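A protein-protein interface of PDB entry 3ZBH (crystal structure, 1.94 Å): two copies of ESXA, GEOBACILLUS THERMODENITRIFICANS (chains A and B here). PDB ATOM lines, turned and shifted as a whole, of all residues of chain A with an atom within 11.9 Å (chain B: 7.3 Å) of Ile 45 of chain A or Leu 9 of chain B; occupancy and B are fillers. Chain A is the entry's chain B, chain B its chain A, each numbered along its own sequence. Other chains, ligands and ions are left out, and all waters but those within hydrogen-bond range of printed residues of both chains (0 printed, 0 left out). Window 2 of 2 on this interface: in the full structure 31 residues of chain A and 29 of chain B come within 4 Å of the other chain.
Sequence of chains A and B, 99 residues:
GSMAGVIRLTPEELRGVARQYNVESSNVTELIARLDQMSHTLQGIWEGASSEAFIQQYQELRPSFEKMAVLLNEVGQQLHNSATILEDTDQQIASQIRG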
ATOM      1  N   ARG A  34       1.149  14.275   5.761  1.00  0.00           N
ATOM      2  CA  ARG A  34       1.148  13.744   7.132  1.00  0.00           C
ATOM      3  C   ARG A  34       2.278  14.302   8.009  1.00  0.00           C
ATOM      4  O   ARG A  34       2.048  14.688   9.175  1.00  0.00           O
ATOM      5  CB  ARG A  34       1.174  12.211   7.158  1.00  0.00           C
ATOM      6  CG  ARG A  34      -0.028  11.527   6.525  1.00  0.00           C
ATOM      7  CD  ARG A  34      -0.011  10.032   6.839  1.00  0.00           C
ATOM      8  NE  ARG A  34       1.202   9.331   6.385  1.00  0.00           N
ATOM      9  CZ  ARG A  34       1.390   8.825   5.164  1.00  0.00           C
ATOM     10  NH1 ARG A  34       0.454   8.940   4.232  1.00  0.00           N
ATOM     11  NH2 ARG A  34       2.521   8.181   4.879  1.00  0.00           N
ATOM     12  N   LEU A  35       3.490  14.346   7.455  1.00  0.00           N
ATOM     13  CA  LEU A  35       4.612  14.985   8.150  1.00  0.00           C
ATOM     14  C   LEU A  35       4.398  16.491   8.373  1.00  0.00           C
ATOM     15  O   LEU A  35       4.851  17.027   9.365  1.00  0.00           O
ATOM     16  CB  LEU A  35       5.921  14.767   7.383  1.00  0.00           C
ATOM     17  CG  LEU A  35       6.351  13.303   7.217  1.00  0.00           C
ATOM     18  CD1 LEU A  35       7.667  13.278   6.435  1.00  0.00           C
ATOM     19  CD2 LEU A  35       6.527  12.646   8.583  1.00  0.00           C
ATOM     20  N   ASP A  36       3.709  17.175   7.463  1.00  0.00           N
ATOM     21  CA  ASP A  36       3.422  18.589   7.693  1.00  0.00           C
ATOM     22  C   ASP A  36       2.579  18.780   8.964  1.00  0.00           C
ATOM     23  O   ASP A  36       2.864  19.661   9.804  1.00  0.00           O
ATOM     24  CB  ASP A  36       2.687  19.227   6.502  1.00  0.00           C
ATOM     25  CG  ASP A  36       3.594  19.532   5.329  1.00  0.00           C
ATOM     26  OD1 ASP A  36       4.857  19.508   5.458  1.00  0.00           O
ATOM     27  OD2 ASP A  36       3.019  19.793   4.255  1.00  0.00           O
ATOM     28  N   GLN A  37       1.567  17.934   9.112  1.00  0.00           N
ATOM     29  CA  GLN A  37       0.701  17.997  10.278  1.00  0.00           C
ATOM     30  C   GLN A  37       1.409  17.514  11.568  1.00  0.00           C
ATOM     31  O   GLN A  37       1.263  18.120  12.645  1.00  0.00           O
ATOM     32  CB  GLN A  37      -0.532  17.152  10.011  1.00  0.00           C
ATOM     33  CG  GLN A  37      -1.531  17.206  11.142  1.00  0.00           C
ATOM     34  CD  GLN A  37      -2.848  16.603  10.728  1.00  0.00           C
ATOM     35  OE1 GLN A  37      -3.044  15.382  10.786  1.00  0.00           O
ATOM     36  NE2 GLN A  37      -3.764  17.459  10.305  1.00  0.00           N
ATOM     37  N   MET A  38       2.165  16.425  11.457  1.00  0.00           N
ATOM     38  CA  MET A  38       3.057  15.979  12.553  1.00  0.00           C
ATOM     39  C   MET A  38       4.029  17.036  13.060  1.00  0.00           C
ATOM     40  O   MET A  38       4.353  17.050  14.268  1.00  0.00           O
ATOM     41  CB  MET A  38       3.808  14.703  12.173  1.00  0.00           C
ATOM     42  CG  MET A  38       2.907  13.478  12.201  1.00  0.00           C
ATOM     43  SD  MET A  38       3.558  12.155  11.187  1.00  0.00           S
ATOM     44  CE  MET A  38       5.068  11.736  12.055  1.00  0.00           C
ATOM     45  N   SER A  39       4.472  17.929  12.175  1.00  0.00           N
ATOM     46  CA  SER A  39       5.321  19.034  12.572  1.00  0.00           C
ATOM     47  C   SER A  39       4.584  20.015  13.482  1.00  0.00           C
ATOM     48  O   SER A  39       5.156  20.511  14.441  1.00  0.00           O
ATOM     49  CB  SER A  39       5.849  19.800  11.360  1.00  0.00           C
ATOM     50  OG  SER A  39       6.935  19.101  10.801  1.00  0.00           O
ATOM     51  N   HIS A  40       3.333  20.320  13.147  1.00  0.00           N
ATOM     52  CA  HIS A  40       2.486  21.157  14.002  1.00  0.00           C
ATOM     53  C   HIS A  40       2.234  20.518  15.328  1.00  0.00           C
ATOM     54  O   HIS A  40       2.341  21.183  16.363  1.00  0.00           O
ATOM     55  CB  HIS A  40       1.154  21.449  13.308  1.00  0.00           C
ATOM     56  CG  HIS A  40       1.264  22.461  12.213  1.00  0.00           C
ATOM     57  ND1 HIS A  40       1.129  22.138  10.910  1.00  0.00           N
ATOM     58  CD2 HIS A  40       1.509  23.829  12.258  1.00  0.00           C
ATOM     59  CE1 HIS A  40       1.292  23.246  10.158  1.00  0.00           C
ATOM     60  NE2 HIS A  40       1.532  24.278  10.986  1.00  0.00           N
ATOM     61  N   THR A  41       1.892  19.233  15.329  1.00  0.00           N
ATOM     62  CA  THR A  41       1.706  18.467  16.574  1.00  0.00           C
ATOM     63  C   THR A  41       2.964  18.580  17.441  1.00  0.00           C
ATOM     64  O   THR A  41       2.893  18.863  18.663  1.00  0.00           O
ATOM     65  CB  THR A  41       1.390  16.984  16.280  1.00  0.00           C
ATOM     66  OG1 THR A  41       0.233  16.898  15.447  1.00  0.00           O
ATOM     67  CG2 THR A  41       1.093  16.212  17.556  1.00  0.00           C
ATOM     68  N   LEU A  42       4.120  18.424  16.802  1.00  0.00           N
ATOM     69  CA  LEU A  42       5.398  18.472  17.527  1.00  0.00           C
ATOM     70  C   LEU A  42       5.655  19.839  18.150  1.00  0.00           C
ATOM     71  O   LEU A  42       6.104  19.925  19.295  1.00  0.00           O
ATOM     72  CB  LEU A  42       6.565  18.090  16.620  1.00  0.00           C
ATOM     73  CG  LEU A  42       7.860  17.737  17.349  1.00  0.00           C
ATOM     74  CD1 LEU A  42       7.648  16.488  18.184  1.00  0.00           C
ATOM     75  CD2 LEU A  42       8.969  17.510  16.331  1.00  0.00           C
ATOM     76  N   GLN A  43       5.356  20.897  17.401  1.00  0.00           N
ATOM     77  CA  GLN A  43       5.431  22.265  17.918  1.00  0.00           C
ATOM     78  C   GLN A  43       4.625  22.507  19.190  1.00  0.00           C
ATOM     79  O   GLN A  43       5.007  23.333  20.007  1.00  0.00           O
ATOM     80  CB  GLN A  43       5.016  23.272  16.851  1.00  0.00           C
ATOM     81  CG  GLN A  43       6.181  23.768  16.030  1.00  0.00           C
ATOM     82  CD  GLN A  43       5.822  24.935  15.135  1.00  0.00           C
ATOM     83  OE1 GLN A  43       4.992  24.817  14.233  1.00  0.00           O
ATOM     84  NE2 GLN A  43       6.468  26.067  15.367  1.00  0.00           N
ATOM     85  N   GLY A  44       3.512  21.799  19.353  1.00  0.00           N
ATOM     86  CA  GLY A  44       2.670  21.969  20.521  1.00  0.00           C
ATOM     87  C   GLY A  44       3.122  21.151  21.716  1.00  0.00           C
ATOM     88  O   GLY A  44       2.861  21.528  22.858  1.00  0.00           O
ATOM     89  N   ILE A  45       3.809  20.037  21.466  1.00  0.00           N
ATOM     90  CA  ILE A  45       4.130  19.101  22.549  1.00  0.00           C
ATOM     91  C   ILE A  45       5.552  19.232  23.113  1.00  0.00           C
ATOM     92  O   ILE A  45       5.828  18.729  24.203  1.00  0.00           O
ATOM     93  CB  ILE A  45       3.773  17.627  22.207  1.00  0.00           C
ATOM     94  CG1 ILE A  45       4.624  17.099  21.060  1.00  0.00           C
ATOM     95  CG2 ILE A  45       2.282  17.490  21.895  1.00  0.00           C
ATOM     96  CD1 ILE A  45       4.375  15.642  20.750  1.00  0.00           C
ATOM     97  N   TRP A  46       6.431  19.913  22.383  1.00  0.00           N
ATOM     98  CA  TRP A  46       7.765  20.237  22.873  1.00  0.00           C
ATOM     99  C   TRP A  46       7.887  21.698  23.008  1.00  0.00           C
ATOM    100  O   TRP A  46       7.130  22.450  22.390  1.00  0.00           O
ATOM    101  CB  TRP A  46       8.859  19.779  21.908  1.00  0.00           C
ATOM    102  CG  TRP A  46       9.300  18.348  22.079  1.00  0.00           C
ATOM    103  CD1 TRP A  46       9.035  17.485  23.143  1.00  0.00           C
ATOM    104  CD2 TRP A  46      10.116  17.562  21.144  1.00  0.00           C
ATOM    105  NE1 TRP A  46       9.595  16.245  22.929  1.00  0.00           N
ATOM    106  CE2 TRP A  46      10.265  16.225  21.750  1.00  0.00           C
ATOM    107  CE3 TRP A  46      10.712  17.816  19.917  1.00  0.00           C
ATOM    108  CZ2 TRP A  46      10.997  15.221  21.135  1.00  0.00           C
ATOM    109  CZ3 TRP A  46      11.436  16.786  19.297  1.00  0.00           C
ATOM    110  CH2 TRP A  46      11.566  15.522  19.890  1.00  0.00           C
ATOM    111  N   GLU A  47       8.874  22.120  23.793  1.00  0.00           N
ATOM    112  CA  GLU A  47       9.263  23.525  23.861  1.00  0.00           C
ATOM    113  C   GLU A  47       9.788  23.987  22.499  1.00  0.00           C
ATOM    114  O   GLU A  47       9.925  23.175  21.574  1.00  0.00           O
ATOM    115  CB  GLU A  47      10.314  23.758  24.957  1.00  0.00           C
ATOM    116  CG  GLU A  47       9.973  23.207  26.342  1.00  0.00           C
ATOM    117  CD  GLU A  47       8.595  23.609  26.854  1.00  0.00           C
ATOM    118  OE1 GLU A  47       8.110  24.722  26.542  1.00  0.00           O
ATOM    119  OE2 GLU A  47       7.994  22.795  27.583  1.00  0.00           O
ATOM    120  N   GLY A  48      10.090  25.284  22.400  1.00  0.00           N
ATOM    121  CA  GLY A  48      10.474  25.932  21.144  1.00  0.00           C
ATOM    122  C   GLY A  48      11.757  25.478  20.464  1.00  0.00           C
ATOM    123  O   GLY A  48      11.797  25.377  19.231  1.00  0.00           O
ATOM    124  N   ALA A  49      12.806  25.210  21.242  1.00  0.00           N
ATOM    125  CA  ALA A  49      14.129  24.902  20.660  1.00  0.00           C
ATOM    126  C   ALA A  49      14.225  23.486  20.095  1.00  0.00           C
ATOM    127  O   ALA A  49      14.788  23.283  19.027  1.00  0.00           O
ATOM    128  CB  ALA A  49      15.251  25.163  21.660  1.00  0.00           C
ATOM    129  N   SER A  50      13.678  22.511  20.813  1.00  0.00           N
ATOM    130  CA  SER A  50      13.606  21.149  20.304  1.00  0.00           C
ATOM    131  C   SER A  50      12.766  21.092  19.009  1.00  0.00           C
ATOM    132  O   SER A  50      13.108  20.367  18.052  1.00  0.00           O
ATOM    133  CB  SER A  50      13.028  20.224  21.370  1.00  0.00           C
ATOM    134  OG  SER A  50      13.919  20.111  22.467  1.00  0.00           O
ATOM    135  N   SER A  51      11.685  21.877  18.996  1.00  0.00           N
ATOM    136  CA  SER A  51      10.817  22.030  17.824  1.00  0.00           C
ATOM    137  C   SER A  51      11.503  22.729  16.656  1.00  0.00           C
ATOM    138  O   SER A  51      11.379  22.289  15.506  1.00  0.00           O
ATOM    139  CB  SER A  51       9.534  22.780  18.201  1.00  0.00           C
ATOM    140  OG  SER A  51       8.643  21.896  18.846  1.00  0.00           O
ATOM    141  N   GLU A  52      12.226  23.806  16.954  1.00  0.00           N
ATOM    142  CA  GLU A  52      12.971  24.565  15.941  1.00  0.00           C
ATOM    143  C   GLU A  52      14.111  23.738  15.311  1.00  0.00           C
ATOM    144  O   GLU A  52      14.525  23.985  14.166  1.00  0.00           O
ATOM    145  CB  GLU A  52      13.500  25.877  16.540  1.00  0.00           C
ATOM    146  CG  GLU A  52      14.201  26.820  15.564  1.00  0.00           C
ATOM    147  CD  GLU A  52      13.491  26.944  14.223  1.00  0.00           C
ATOM    148  OE1 GLU A  52      12.314  27.370  14.193  1.00  0.00           O
ATOM    149  OE2 GLU A  52      14.117  26.601  13.193  1.00  0.00           O
ATOM    150  N   PHE A  54      13.960  20.357  14.777  1.00  0.00           N
ATOM    151  CA  PHE A  54      13.297  19.506  13.803  1.00  0.00           C
ATOM    152  C   PHE A  54      12.834  20.274  12.573  1.00  0.00           C
ATOM    153  O   PHE A  54      13.075  19.819  11.465  1.00  0.00           O
ATOM    154  CB  PHE A  54      12.141  18.700  14.407  1.00  0.00           C
ATOM    155  CG  PHE A  54      11.341  17.942  13.379  1.00  0.00           C
ATOM    156  CD1 PHE A  54      11.800  16.736  12.871  1.00  0.00           C
ATOM    157  CD2 PHE A  54      10.139  18.452  12.897  1.00  0.00           C
ATOM    158  CE1 PHE A  54      11.078  16.042  11.913  1.00  0.00           C
ATOM    159  CE2 PHE A  54       9.413  17.763  11.937  1.00  0.00           C
ATOM    160  CZ  PHE A  54       9.879  16.554  11.446  1.00  0.00           C
ATOM    161  N   ILE A  55      12.176  21.422  12.764  1.00  0.00           N
ATOM    162  CA  ILE A  55      11.541  22.165  11.654  1.00  0.00           C
ATOM    163  C   ILE A  55      12.499  22.637  10.593  1.00  0.00           C
ATOM    164  O   ILE A  55      12.170  22.622   9.407  1.00  0.00           O
ATOM    165  CB  ILE A  55      10.730  23.388  12.135  1.00  0.00           C
ATOM    166  CG1 ILE A  55       9.343  22.948  12.576  1.00  0.00           C
ATOM    167  CG2 ILE A  55      10.591  24.446  11.040  1.00  0.00           C
ATOM    168  CD1 ILE A  55       8.556  24.056  13.243  1.00  0.00           C
ATOM    169  N   LEU B   9      -0.413  17.583  28.903  1.00  0.00           N
ATOM    170  CA  LEU B   9       0.246  16.562  28.018  1.00  0.00           C
ATOM    171  C   LEU B   9       0.802  15.379  28.818  1.00  0.00           C
ATOM    172  O   LEU B   9       1.548  15.566  29.789  1.00  0.00           O
ATOM    173  CB  LEU B   9       1.337  17.197  27.140  1.00  0.00           C
ATOM    174  CG  LEU B   9       2.707  17.586  27.721  1.00  0.00           C
ATOM    175  CD1 LEU B   9       3.754  17.590  26.612  1.00  0.00           C
ATOM    176  CD2 LEU B   9       2.667  18.929  28.441  1.00  0.00           C
ATOM    177  N   THR B  10       0.438  14.173  28.381  1.00  0.00           N
ATOM    178  CA  THR B  10       0.688  12.932  29.127  1.00  0.00           C
ATOM    179  C   THR B  10       1.738  12.043  28.453  1.00  0.00           C
ATOM    180  O   THR B  10       1.934  12.139  27.238  1.00  0.00           O
ATOM    181  CB  THR B  10      -0.608  12.107  29.266  1.00  0.00           C
ATOM    182  OG1 THR B  10      -0.980  11.594  27.984  1.00  0.00           O
ATOM    183  CG2 THR B  10      -1.754  12.957  29.825  1.00  0.00           C
ATOM    184  N   PRO B  11       2.409  11.165  29.232  1.00  0.00           N
ATOM    185  CA  PRO B  11       3.295  10.184  28.600  1.00  0.00           C
ATOM    186  C   PRO B  11       2.571   9.420  27.490  1.00  0.00           C
ATOM    187  O   PRO B  11       3.179   9.088  26.476  1.00  0.00           O
ATOM    188  CB  PRO B  11       3.672   9.248  29.759  1.00  0.00           C
ATOM    189  CG  PRO B  11       3.600  10.130  30.970  1.00  0.00           C
ATOM    190  CD  PRO B  11       2.451  11.072  30.709  1.00  0.00           C
ATOM    191  N   GLU B  12       1.274   9.174  27.668  1.00  0.00           N
ATOM    192  CA  GLU B  12       0.488   8.487  26.640  1.00  0.00           C
ATOM    193  C   GLU B  12       0.340   9.266  25.334  1.00  0.00           C
ATOM    194  O   GLU B  12       0.485   8.690  24.259  1.00  0.00           O
ATOM    195  CB  GLU B  12      -0.857   8.009  27.188  1.00  0.00           C
ATOM    196  CG  GLU B  12      -0.739   6.672  27.908  1.00  0.00           C
ATOM    197  CD  GLU B  12       0.259   5.732  27.238  1.00  0.00           C
ATOM    198  OE1 GLU B  12      -0.020   5.262  26.115  1.00  0.00           O
ATOM    199  OE2 GLU B  12       1.333   5.472  27.828  1.00  0.00           O
ATOM    200  N   GLU B  13       0.053  10.563  25.441  1.00  0.00           N
ATOM    201  CA  GLU B  13       0.073  11.467  24.285  1.00  0.00           C
ATOM    202  C   GLU B  13       1.412  11.363  23.559  1.00  0.00           C
ATOM    203  O   GLU B  13       1.451  11.078  22.354  1.00  0.00           O
ATOM    204  CB  GLU B  13      -0.188  12.927  24.694  1.00  0.00           C
ATOM    205  CG  GLU B  13      -1.650  13.369  24.614  1.00  0.00           C
ATOM    206  CD  GLU B  13      -2.353  13.387  25.968  1.00  0.00           C
ATOM    207  OE1 GLU B  13      -1.938  14.175  26.849  1.00  0.00           O
ATOM    208  OE2 GLU B  13      -3.312  12.605  26.162  1.00  0.00           O
ATOM    209  N   LEU B  14       2.497  11.559  24.313  1.00  0.00           N
ATOM    210  CA  LEU B  14       3.854  11.566  23.768  1.00  0.00           C
ATOM    211  C   LEU B  14       4.217  10.272  23.056  1.00  0.00           C
ATOM    212  O   LEU B  14       4.826  10.303  21.986  1.00  0.00           O
ATOM    213  CB  LEU B  14       4.875  11.866  24.864  1.00  0.00           C
ATOM    214  CG  LEU B  14       4.982  13.300  25.384  1.00  0.00           C
ATOM    215  CD1 LEU B  14       5.752  13.314  26.695  1.00  0.00           C
ATOM    216  CD2 LEU B  14       5.630  14.254  24.382  1.00  0.00           C
ATOM    217  N   ARG B  15       3.845   9.136  23.642  1.00  0.00           N
ATOM    218  CA  ARG B  15       4.108   7.837  23.021  1.00  0.00           C
ATOM    219  C   ARG B  15       3.339   7.627  21.725  1.00  0.00           C
ATOM    220  O   ARG B  15       3.859   7.013  20.797  1.00  0.00           O
ATOM    221  CB  ARG B  15       3.829   6.696  23.992  1.00  0.00           C
ATOM    222  CG  ARG B  15       4.966   6.478  24.968  1.00  0.00           C
ATOM    223  CD  ARG B  15       4.657   5.353  25.938  1.00  0.00           C
ATOM    224  NE  ARG B  15       5.668   5.332  26.982  1.00  0.00           N
ATOM    225  CZ  ARG B  15       5.414   5.443  28.280  1.00  0.00           C
ATOM    226  NH1 ARG B  15       4.159   5.563  28.708  1.00  0.00           N
ATOM    227  NH2 ARG B  15       6.422   5.436  29.146  1.00  0.00           N
ATOM    228  N   VAL B  17       2.452  10.049  19.637  1.00  0.00           N
ATOM    229  CA  VAL B  17       3.184  10.850  18.655  1.00  0.00           C
ATOM    230  C   VAL B  17       4.531  10.203  18.290  1.00  0.00           C
ATOM    231  O   VAL B  17       4.947  10.254  17.127  1.00  0.00           O
ATOM    232  CB  VAL B  17       3.342  12.323  19.107  1.00  0.00           C
ATOM    233  CG1 VAL B  17       4.025  13.162  18.033  1.00  0.00           C
ATOM    234  CG2 VAL B  17       1.971  12.936  19.416  1.00  0.00           C
ATOM    235  N   ALA B  18       5.194   9.591  19.271  1.00  0.00           N
ATOM    236  CA  ALA B  18       6.458   8.911  19.051  1.00  0.00           C
ATOM    237  C   ALA B  18       6.324   7.825  17.969  1.00  0.00           C
ATOM    238  O   ALA B  18       7.139   7.763  17.048  1.00  0.00           O
ATOM    239  CB  ALA B  18       6.980   8.313  20.352  1.00  0.00           C
ATOM    240  N   TYR B  21       5.900   9.066  14.342  1.00  0.00           N
ATOM    241  CA  TYR B  21       7.240   9.336  13.796  1.00  0.00           C
ATOM    242  C   TYR B  21       8.009   8.070  13.417  1.00  0.00           C
ATOM    243  O   TYR B  21       8.664   8.038  12.365  1.00  0.00           O
ATOM    244  CB  TYR B  21       8.065  10.250  14.715  1.00  0.00           C
ATOM    245  CG  TYR B  21       7.778  11.717  14.500  1.00  0.00           C
ATOM    246  CD1 TYR B  21       8.459  12.446  13.519  1.00  0.00           C
ATOM    247  CD2 TYR B  21       6.792  12.383  15.252  1.00  0.00           C
ATOM    248  CE1 TYR B  21       8.193  13.786  13.290  1.00  0.00           C
ATOM    249  CE2 TYR B  21       6.517  13.723  15.023  1.00  0.00           C
ATOM    250  CZ  TYR B  21       7.196  14.416  14.048  1.00  0.00           C
ATOM    251  OH  TYR B  21       6.943  15.746  13.823  1.00  0.00           O
ATOM    252  N   LEU B  79      10.934  11.357  21.574  1.00  0.00           N
ATOM    253  CA  LEU B  79       9.573  11.454  22.115  1.00  0.00           C
ATOM    254  C   LEU B  79       9.345  10.305  23.097  1.00  0.00           C
ATOM    255  O   LEU B  79       8.855  10.522  24.216  1.00  0.00           O
ATOM    256  CB  LEU B  79       8.524  11.475  20.987  1.00  0.00           C
ATOM    257  CG  LEU B  79       8.469  12.791  20.198  1.00  0.00           C
ATOM    258  CD1 LEU B  79       7.723  12.632  18.880  1.00  0.00           C
ATOM    259  CD2 LEU B  79       7.817  13.890  21.034  1.00  0.00           C
ATOM    260  N   SER B  82      11.258  11.208  26.241  1.00  0.00           N
ATOM    261  CA  SER B  82      10.480  12.218  26.992  1.00  0.00           C
ATOM    262  C   SER B  82       9.334  11.626  27.799  1.00  0.00           C
ATOM    263  O   SER B  82       9.127  11.996  28.972  1.00  0.00           O
ATOM    264  CB  SER B  82       9.910  13.271  26.041  1.00  0.00           C
ATOM    265  OG  SER B  82      10.948  13.860  25.303  1.00  0.00           O
ATOM    266  N   LEU B  86       8.935  11.880  31.883  1.00  0.00           N
ATOM    267  CA  LEU B  86       7.768  12.506  32.466  1.00  0.00           C
ATOM    268  C   LEU B  86       6.999  11.545  33.385  1.00  0.00           C
ATOM    269  O   LEU B  86       6.528  11.939  34.469  1.00  0.00           O
ATOM    270  CB  LEU B  86       6.864  13.001  31.331  1.00  0.00           C
ATOM    271  CG  LEU B  86       5.471  13.546  31.635  1.00  0.00           C
ATOM    272  CD1 LEU B  86       5.541  14.714  32.620  1.00  0.00           C
ATOM    273  CD2 LEU B  86       4.790  13.954  30.331  1.00  0.00           C
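No position is printed for both chains. Of the 11 pairs that touch across the chains among the printed residues, none has its exchanged pair printed and touching as well.
Among the printed residues, pairs that only touch across the chains: Ile 45 of chain A with Leu 9 of chain B (3.4 Å), Trp 46 of chain A with Leu 79 of chain B (3.4 Å), Trp 46 of chain A with Ser 82 of chain B (3.6 Å), Leu 42 of chain A with Tyr 21 of chain B (3.7 Å), Ser 39 of chain A with Tyr 21 of chain B (3.7 Å), Ile 45 of chain A with Val 17 of chain B (3.7 Å), Phe 54 of chain A with Tyr 21 of chain B (3.7 Å), Leu 42 of chain A with Leu 79 of chain B (3.9 Å), Thr 41 of chain A with Val 17 of chain B (3.9 Å) and Ile 45 of chain A with Leu 79 of chain B (3.9 Å).
Of the 13 printed residues of chain B, 5 touch a printed residue of chain A. Hydrophobic or aromatic side chains of chain B within 4 Å of the printed part of chain A: Leu 9, Val 17, Tyr 21 and Leu 79. Among the printed residues, 11 pairs touch across the chains.
The backbone carbonyl oxygen (O) of Leu 35 of chain A sits at hydrogen-bond distance from the side-chain hydroxyl (OG) of Ser 39 of chain A, at 3.3 Å. The side-chain hydroxyl (OG1) of Thr 41 of chain A is in hydrogen-bond range of the backbone carbonyl oxygen (O) of Gln 37 of chain A, at 3.2 Å. O of Leu 42 of chain A is in hydrogen-bond range of OG of Ser 51 of chain A (3.2 Å).
Ile 45 of chain A touches just these residues of chain B: Leu 9 (3.4 Å), Val 17 (3.7 Å) and Leu 79 (3.9 Å). Leu 9 of chain B touches just one residue of chain A: Ile 45 (3.4 Å). No residue of chain B comes within 4 Å of Gly 44 of chain A. No residue of chain A comes within 4 Å of Glu 13 of chain B. No residue of chain A comes within 4 Å of Leu 14 of chain B. Val 17 of chain B touches two residues of chain A. Of the printed residues of chain B, Trp 46 of chain A touches Leu 79 and Ser 82. Of the printed residues of chain B, Ser 39 of chain A touches Tyr 21 (3.7 Å). Printed residues of chain B within 4 Å of Met 38 of chain A: Tyr 21. Of the printed residues of chain A, Leu 79 of chain B touches Leu 42, Ile 45 and Trp 46. Gln 43 of chain A touches none of the printed residues of chain B. The nearest printed residue of chain A that does not touch Leu 9 of chain B is Gly 44 of chain A (5.5 Å). The nearest printed residue of chain A that does not touch Leu 79 of chain B is Met 38 of chain A (7.2 Å).
The side-chain hydroxyl of Tyr 21 of chain B sits at hydrogen-bond distance from the backbone carbonyl oxygen of Met 38 of chain A (2.9 Å).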
